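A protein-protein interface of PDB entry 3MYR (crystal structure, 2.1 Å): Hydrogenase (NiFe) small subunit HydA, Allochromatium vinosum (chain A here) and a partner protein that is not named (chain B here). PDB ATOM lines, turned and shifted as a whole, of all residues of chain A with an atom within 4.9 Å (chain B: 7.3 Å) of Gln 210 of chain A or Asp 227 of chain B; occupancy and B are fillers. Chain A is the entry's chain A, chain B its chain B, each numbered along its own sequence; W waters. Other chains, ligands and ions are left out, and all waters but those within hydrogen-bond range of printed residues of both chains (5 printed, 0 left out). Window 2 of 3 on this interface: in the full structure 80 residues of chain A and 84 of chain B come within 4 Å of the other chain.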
ATOM      1  N   GLU A 206       1.100 -25.503  -0.599  1.00  0.00           N
ATOM      2  CA  GLU A 206       0.286 -26.704  -0.845  1.00  0.00           C
ATOM      3  C   GLU A 206       0.530 -27.784   0.240  1.00  0.00           C
ATOM      4  O   GLU A 206      -0.407 -28.333   0.772  1.00  0.00           O
ATOM      5  CB  GLU A 206       0.565 -27.258  -2.279  1.00  0.00           C
ATOM      6  CG  GLU A 206      -0.286 -28.461  -2.616  1.00  0.00           C
ATOM      7  CD  GLU A 206      -1.828 -28.174  -2.637  1.00  0.00           C
ATOM      8  OE1 GLU A 206      -2.598 -29.154  -2.791  1.00  0.00           O
ATOM      9  OE2 GLU A 206      -2.275 -26.997  -2.504  1.00  0.00           O
ATOM     10  N   GLY A 207       1.781 -28.052   0.607  1.00  0.00           N
ATOM     11  CA  GLY A 207       2.111 -29.086   1.571  1.00  0.00           C
ATOM     12  C   GLY A 207       1.518 -28.707   2.940  1.00  0.00           C
ATOM     13  O   GLY A 207       0.973 -29.549   3.635  1.00  0.00           O
ATOM     14  N   ALA A 208       1.613 -27.436   3.338  1.00  0.00           N
ATOM     15  CA  ALA A 208       1.038 -27.038   4.630  1.00  0.00           C
ATOM     16  C   ALA A 208      -0.462 -27.294   4.619  1.00  0.00           C
ATOM     17  O   ALA A 208      -1.010 -27.814   5.583  1.00  0.00           O
ATOM     18  CB  ALA A 208       1.323 -25.495   4.935  1.00  0.00           C
ATOM     19  N   LYS A 209      -1.126 -26.906   3.533  1.00  0.00           N
ATOM     20  CA  LYS A 209      -2.606 -27.009   3.492  1.00  0.00           C
ATOM     21  C   LYS A 209      -3.030 -28.434   3.489  1.00  0.00           C
ATOM     22  O   LYS A 209      -4.100 -28.757   4.006  1.00  0.00           O
ATOM     23  CB  LYS A 209      -3.197 -26.375   2.218  1.00  0.00           C
ATOM     24  CG  LYS A 209      -3.106 -24.828   2.222  1.00  0.00           C
ATOM     25  CD  LYS A 209      -3.598 -24.384   0.817  1.00  0.00           C
ATOM     26  CE  LYS A 209      -3.386 -22.921   0.469  1.00  0.00           C
ATOM     27  NZ  LYS A 209      -3.936 -22.097   1.449  1.00  0.00           N
ATOM     28  N   GLN A 210      -2.190 -29.298   2.923  1.00  0.00           N
ATOM     29  CA  GLN A 210      -2.514 -30.717   2.825  1.00  0.00           C
ATOM     30  C   GLN A 210      -2.026 -31.539   4.027  1.00  0.00           C
ATOM     31  O   GLN A 210      -2.266 -32.750   4.062  1.00  0.00           O
ATOM     32  CB  GLN A 210      -1.876 -31.339   1.575  1.00  0.00           C
ATOM     33  CG  GLN A 210      -2.439 -30.678   0.307  1.00  0.00           C
ATOM     34  CD  GLN A 210      -3.882 -31.109   0.076  1.00  0.00           C
ATOM     35  OE1 GLN A 210      -4.153 -32.286   0.057  1.00  0.00           O
ATOM     36  NE2 GLN A 210      -4.810 -30.152  -0.018  1.00  0.00           N
ATOM     37  N   GLY A 211      -1.405 -30.938   5.019  1.00  0.00           N
ATOM     38  CA  GLY A 211      -0.897 -31.789   6.082  1.00  0.00           C
ATOM     39  C   GLY A 211       0.318 -32.625   5.722  1.00  0.00           C
ATOM     40  O   GLY A 211       0.524 -33.696   6.304  1.00  0.00           O
ATOM     41  N   TRP A 212       1.191 -32.111   4.853  1.00  0.00           N
ATOM     42  CA  TRP A 212       2.512 -32.729   4.663  1.00  0.00           C
ATOM     43  C   TRP A 212       3.373 -32.415   5.874  1.00  0.00           C
ATOM     44  O   TRP A 212       3.061 -31.535   6.650  1.00  0.00           O
ATOM     45  CB  TRP A 212       3.181 -32.253   3.366  1.00  0.00           C
ATOM     46  CG  TRP A 212       2.365 -32.612   2.118  1.00  0.00           C
ATOM     47  CD1 TRP A 212       1.184 -33.359   2.066  1.00  0.00           C
ATOM     48  CD2 TRP A 212       2.675 -32.269   0.744  1.00  0.00           C
ATOM     49  NE1 TRP A 212       0.758 -33.480   0.742  1.00  0.00           N
ATOM     50  CE2 TRP A 212       1.628 -32.794  -0.076  1.00  0.00           C
ATOM     51  CE3 TRP A 212       3.701 -31.520   0.139  1.00  0.00           C
ATOM     52  CZ2 TRP A 212       1.596 -32.593  -1.470  1.00  0.00           C
ATOM     53  CZ3 TRP A 212       3.674 -31.318  -1.229  1.00  0.00           C
ATOM     54  CH2 TRP A 212       2.612 -31.834  -2.020  1.00  0.00           C
ATOM     55  N   SER B 224      -1.762 -21.652  11.120  1.00  0.00           N
ATOM     56  CA  SER B 224      -2.877 -22.533  10.707  1.00  0.00           C
ATOM     57  C   SER B 224      -3.376 -22.203   9.290  1.00  0.00           C
ATOM     58  O   SER B 224      -3.978 -21.173   9.089  1.00  0.00           O
ATOM     59  CB  SER B 224      -4.034 -22.238  11.638  1.00  0.00           C
ATOM     60  OG  SER B 224      -4.332 -20.839  11.636  1.00  0.00           O
ATOM     61  N   PRO B 225      -3.175 -23.095   8.317  1.00  0.00           N
ATOM     62  CA  PRO B 225      -3.630 -22.720   6.972  1.00  0.00           C
ATOM     63  C   PRO B 225      -5.119 -22.995   6.796  1.00  0.00           C
ATOM     64  O   PRO B 225      -5.751 -23.657   7.654  1.00  0.00           O
ATOM     65  CB  PRO B 225      -2.788 -23.647   6.034  1.00  0.00           C
ATOM     66  CG  PRO B 225      -2.438 -24.840   6.932  1.00  0.00           C
ATOM     67  CD  PRO B 225      -2.471 -24.386   8.365  1.00  0.00           C
ATOM     68  N   ILE B 226      -5.681 -22.453   5.713  1.00  0.00           N
ATOM     69  CA  ILE B 226      -7.107 -22.595   5.411  1.00  0.00           C
ATOM     70  C   ILE B 226      -7.174 -23.363   4.103  1.00  0.00           C
ATOM     71  O   ILE B 226      -6.494 -23.001   3.104  1.00  0.00           O
ATOM     72  CB  ILE B 226      -7.760 -21.197   5.219  1.00  0.00           C
ATOM     73  CG1 ILE B 226      -7.747 -20.388   6.554  1.00  0.00           C
ATOM     74  CG2 ILE B 226      -9.150 -21.375   4.683  1.00  0.00           C
ATOM     75  CD1 ILE B 226      -8.017 -18.861   6.362  1.00  0.00           C
ATOM     76  N   ASP B 227      -7.874 -24.481   4.109  1.00  0.00           N
ATOM     77  CA  ASP B 227      -8.131 -25.190   2.833  1.00  0.00           C
ATOM     78  C   ASP B 227      -9.405 -25.975   3.068  1.00  0.00           C
ATOM     79  O   ASP B 227      -9.442 -26.974   3.812  1.00  0.00           O
ATOM     80  CB  ASP B 227      -6.990 -26.171   2.523  1.00  0.00           C
ATOM     81  CG  ASP B 227      -7.168 -26.878   1.113  1.00  0.00           C
ATOM     82  OD1 ASP B 227      -8.305 -27.063   0.615  1.00  0.00           O
ATOM     83  OD2 ASP B 227      -6.170 -27.342   0.552  1.00  0.00           O
ATOM     84  N   LEU B 228     -10.450 -25.550   2.408  1.00  0.00           N
ATOM     85  CA  LEU B 228     -11.754 -26.120   2.618  1.00  0.00           C
ATOM     86  C   LEU B 228     -11.811 -27.592   2.217  1.00  0.00           C
ATOM     87  O   LEU B 228     -12.800 -28.277   2.542  1.00  0.00           O
ATOM     88  CB  LEU B 228     -12.735 -25.369   1.743  1.00  0.00           C
ATOM     89  CG  LEU B 228     -13.320 -24.066   2.329  1.00  0.00           C
ATOM     90  CD1 LEU B 228     -12.847 -23.484   3.672  1.00  0.00           C
ATOM     91  CD2 LEU B 228     -14.065 -23.095   1.318  1.00  0.00           C
ATOM     92  N   ASP B 229     -10.862 -28.021   1.367  1.00  0.00           N
ATOM     93  CA  ASP B 229     -10.915 -29.372   0.823  1.00  0.00           C
ATOM     94  C   ASP B 229      -9.873 -30.261   1.439  1.00  0.00           C
ATOM     95  O   ASP B 229      -9.519 -31.273   0.897  1.00  0.00           O
ATOM     96  CB  ASP B 229     -10.849 -29.287  -0.699  1.00  0.00           C
ATOM     97  CG  ASP B 229     -12.113 -28.563  -1.231  1.00  0.00           C
ATOM     98  OD1 ASP B 229     -11.968 -27.435  -1.729  1.00  0.00           O
ATOM     99  OD2 ASP B 229     -13.279 -29.033  -0.981  1.00  0.00           O
ATOM    100  N   SER B 230      -9.435 -29.914   2.646  1.00  0.00           N
ATOM    101  CA  SER B 230      -8.367 -30.666   3.244  1.00  0.00           C
ATOM    102  C   SER B 230      -8.770 -31.268   4.584  1.00  0.00           C
ATOM    103  O   SER B 230      -9.376 -30.610   5.407  1.00  0.00           O
ATOM    104  CB  SER B 230      -7.185 -29.715   3.540  1.00  0.00           C
ATOM    105  OG  SER B 230      -6.157 -30.391   4.206  1.00  0.00           O
ATOM    106  N   ASP B 231      -8.179 -32.420   4.866  1.00  0.00           N
ATOM    107  CA  ASP B 231      -8.274 -33.055   6.161  1.00  0.00           C
ATOM    108  C   ASP B 231      -7.348 -32.496   7.196  1.00  0.00           C
ATOM    109  O   ASP B 231      -7.407 -32.989   8.314  1.00  0.00           O
ATOM    110  CB  ASP B 231      -8.078 -34.597   6.111  1.00  0.00           C
ATOM    111  CG  ASP B 231      -6.551 -35.050   5.924  1.00  0.00           C
ATOM    112  OD1 ASP B 231      -5.693 -34.278   5.368  1.00  0.00           O
ATOM    113  OD2 ASP B 231      -6.204 -36.204   6.354  1.00  0.00           O
ATOM    114  N   SER B 232      -6.506 -31.524   6.858  1.00  0.00           N
ATOM    115  CA  SER B 232      -5.456 -31.066   7.811  1.00  0.00           C
ATOM    116  C   SER B 232      -5.306 -29.530   7.831  1.00  0.00           C
ATOM    117  O   SER B 232      -4.133 -28.966   7.881  1.00  0.00           O
ATOM    118  CB  SER B 232      -4.100 -31.631   7.404  1.00  0.00           C
ATOM    119  OG  SER B 232      -3.085 -31.162   8.318  1.00  0.00           O
ATOM    120  N   ALA B 233      -6.407 -28.848   7.566  1.00  0.00           N
ATOM    121  CA  ALA B 233      -6.432 -27.391   7.506  1.00  0.00           C
ATOM    122  C   ALA B 233      -7.775 -26.900   8.052  1.00  0.00           C
ATOM    123  O   ALA B 233      -8.698 -27.663   8.229  1.00  0.00           O
ATOM    124  CB  ALA B 233      -6.284 -26.897   6.045  1.00  0.00           C
ATOM    125  N   LEU B 234      -7.894 -25.597   8.252  1.00  0.00           N
ATOM    126  CA  LEU B 234      -9.189 -25.021   8.657  1.00  0.00           C
ATOM    127  C   LEU B 234     -10.136 -25.168   7.490  1.00  0.00           C
ATOM    128  O   LEU B 234      -9.804 -24.726   6.380  1.00  0.00           O
ATOM    129  CB  LEU B 234      -9.019 -23.562   8.922  1.00  0.00           C
ATOM    130  CG  LEU B 234      -8.530 -23.058  10.263  1.00  0.00           C
ATOM    131  CD1 LEU B 234      -8.549 -23.982  11.554  1.00  0.00           C
ATOM    132  CD2 LEU B 234      -7.513 -21.894  10.256  1.00  0.00           C
ATOM    133  N   ASN B 235     -11.294 -25.786   7.727  1.00  0.00           N
ATOM    134  CA  ASN B 235     -12.265 -26.104   6.683  1.00  0.00           C
ATOM    135  C   ASN B 235     -13.670 -25.823   7.292  1.00  0.00           C
ATOM    136  O   ASN B 235     -13.769 -25.199   8.395  1.00  0.00           O
ATOM    137  CB  ASN B 235     -12.105 -27.555   6.192  1.00  0.00           C
ATOM    138  CG  ASN B 235     -12.178 -28.578   7.328  1.00  0.00           C
ATOM    139  OD1 ASN B 235     -11.565 -29.656   7.276  1.00  0.00           O
ATOM    140  ND2 ASN B 235     -12.875 -28.218   8.372  1.00  0.00           N
ATOM    141  N   ALA B 236     -14.748 -26.184   6.598  1.00  0.00           N
ATOM    142  CA  ALA B 236     -16.105 -25.816   7.082  1.00  0.00           C
ATOM    143  C   ALA B 236     -16.422 -26.419   8.455  1.00  0.00           C
ATOM    144  O   ALA B 236     -17.029 -25.767   9.305  1.00  0.00           O
ATOM    145  CB  ALA B 236     -17.180 -26.248   6.068  1.00  0.00           C
ATOM    146  N   VAL B 455     -12.549 -15.765   2.922  1.00  0.00           N
ATOM    147  CA  VAL B 455     -12.263 -17.106   2.419  1.00  0.00           C
ATOM    148  C   VAL B 455     -13.200 -17.473   1.251  1.00  0.00           C
ATOM    149  O   VAL B 455     -12.731 -17.889   0.178  1.00  0.00           O
ATOM    150  CB  VAL B 455     -12.376 -18.133   3.534  1.00  0.00           C
ATOM    151  CG1 VAL B 455     -12.407 -19.550   2.962  1.00  0.00           C
ATOM    152  CG2 VAL B 455     -11.217 -17.964   4.493  1.00  0.00           C
ATOM    153  N   THR B 460      -7.379 -17.406   0.529  1.00  0.00           N
ATOM    154  CA  THR B 460      -7.149 -18.344   1.631  1.00  0.00           C
ATOM    155  C   THR B 460      -5.714 -18.201   2.142  1.00  0.00           C
ATOM    156  O   THR B 460      -5.196 -19.079   2.809  1.00  0.00           O
ATOM    157  CB  THR B 460      -7.424 -19.797   1.228  1.00  0.00           C
ATOM    158  OG1 THR B 460      -6.606 -20.142   0.109  1.00  0.00           O
ATOM    159  CG2 THR B 460      -8.851 -20.010   0.807  1.00  0.00           C
HETATM  160  O   HOH W   1      -3.636 -19.481   0.026  1.00  0.00           O
HETATM  161  O   HOH W   2      -3.759 -20.795   4.211  1.00  0.00           O
HETATM  162  O   HOH W   3      -4.770 -33.590   2.874  1.00  0.00           O
HETATM  163  O   HOH W   4      -7.067 -23.064   0.262  1.00  0.00           O
HETATM  164  O   HOH W   5      -7.680 -31.737  -0.836  1.00  0.00           O
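OG of Ser 230 of chain B lies within hydrogen-bond range of O of Lys 209 of chain A, 2.6 Å away. The backbone carbonyl oxygen (O) of Ile 226 of chain B is in hydrogen-bond range of the side-chain amino group (NZ) of Lys 209 of chain A. NE2 of Gln 210 of chain A is in hydrogen-bond range of OD2 of Asp 227 of chain B.
OD1 of Asp 227 of chain B sits at hydrogen-bond distance from N of Asp 229 of chain B (2.8 Å). O of Leu 234 of chain B sits at hydrogen-bond distance from N of Asp 227 of chain B (3.0 Å). OG of Ser 230 of chain B sits at hydrogen-bond distance from N of Ser 232 of chain B (2.9 Å). The backbone carbonyl oxygen of Pro 225 of chain B sits at hydrogen-bond distance from the backbone NH of Leu 234 of chain B, 3.0 Å away. O of Ser 230 of chain B sits close to OD1 of Asn 235 of chain B, 3.0 Å away.
Pro 225 of chain B touches Ala 208 of chain A. Asp 227 of chain B touches Lys 209 of chain A (OD2 to CB, 3.5 Å). O of Ser 232 of chain B touches O of Lys 209 of chain A (3.9 Å). Lys 209 of chain A touches Ala 233 of chain B (O to CB, 3.5 Å). NZ of Lys 209 of chain A touches O of Thr 460 of chain B, 3.5 Å away. Ser 230 of chain B touches Gln 210 of chain A (OG to CA, 3.9 Å). Gln 210 of chain A touches Asp 231 of chain B. Gln 210 of chain A touches Ser 232 of chain B. CA of Gly 211 of chain A touches OG of Ser 232 of chain B, 3.2 Å away.
Gln 210 of chain A touches just these residues of chain B: Asp 227, Ser 230, Asp 231 and Ser 232. Of chain A, only Lys 209 and Gln 210 come within 4 Å of Asp 227 of chain B. Printed residues of chain A within 4 Å of Ser 230 of chain B: Lys 209 and Gln 210. Of the printed residues of chain B, Lys 209 of chain A touches Ile 226, Asp 227, Ser 230, Ser 232, Ala 233 and Thr 460. Printed residues of chain B within 4 Å of Ala 208 of chain A: Pro 225 (3.6 Å). Ala 236 of chain B touches none of the printed residues of chain A. The nearest residue of chain B that does not touch Gln 210 of chain A is Asp 229 of chain B (4.9 Å). The nearest printed residue of chain A that does not touch Asp 227 of chain B is Glu 206 of chain A (5.0 Å). The nearest printed residue of chain B that does not touch Lys 209 of chain A is Pro 225 of chain B (4.003 Å).
Printed residues of chain A that touch a printed residue of chain B: Ala 208, Lys 209, Gln 210 and Gly 211.
Water W5 bridges O of Asp 229 of chain B (2.6 Å) and NE2 of Gln 210 of chain A (3.4 Å). Water W2 lies within hydrogen-bond range of O of Thr 460 of chain B (2.6 Å), N of Ile 226 of chain B (2.9 Å) and NZ of Lys 209 of chain A (3.1 Å). Water W3 bridges the side-chain carboxylate (OD1) of Asp 231 of chain B (2.7 Å) and the backbone carbonyl oxygen (O) of Gln 210 of chain A (2.9 Å). Water W4 lies within hydrogen-bond range of the backbone carbonyl oxygen of Ile 226 of chain B (2.9 Å), the side-chain hydroxyl of Thr 460 of chain B (3.0 Å) and the side-chain amino group of Lys 209 of chain A (3.5 Å). Water W1 bridges NZ of Lys 209 of chain A (3.0 Å) and OG1 of Thr 460 of chain B (3.0 Å).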
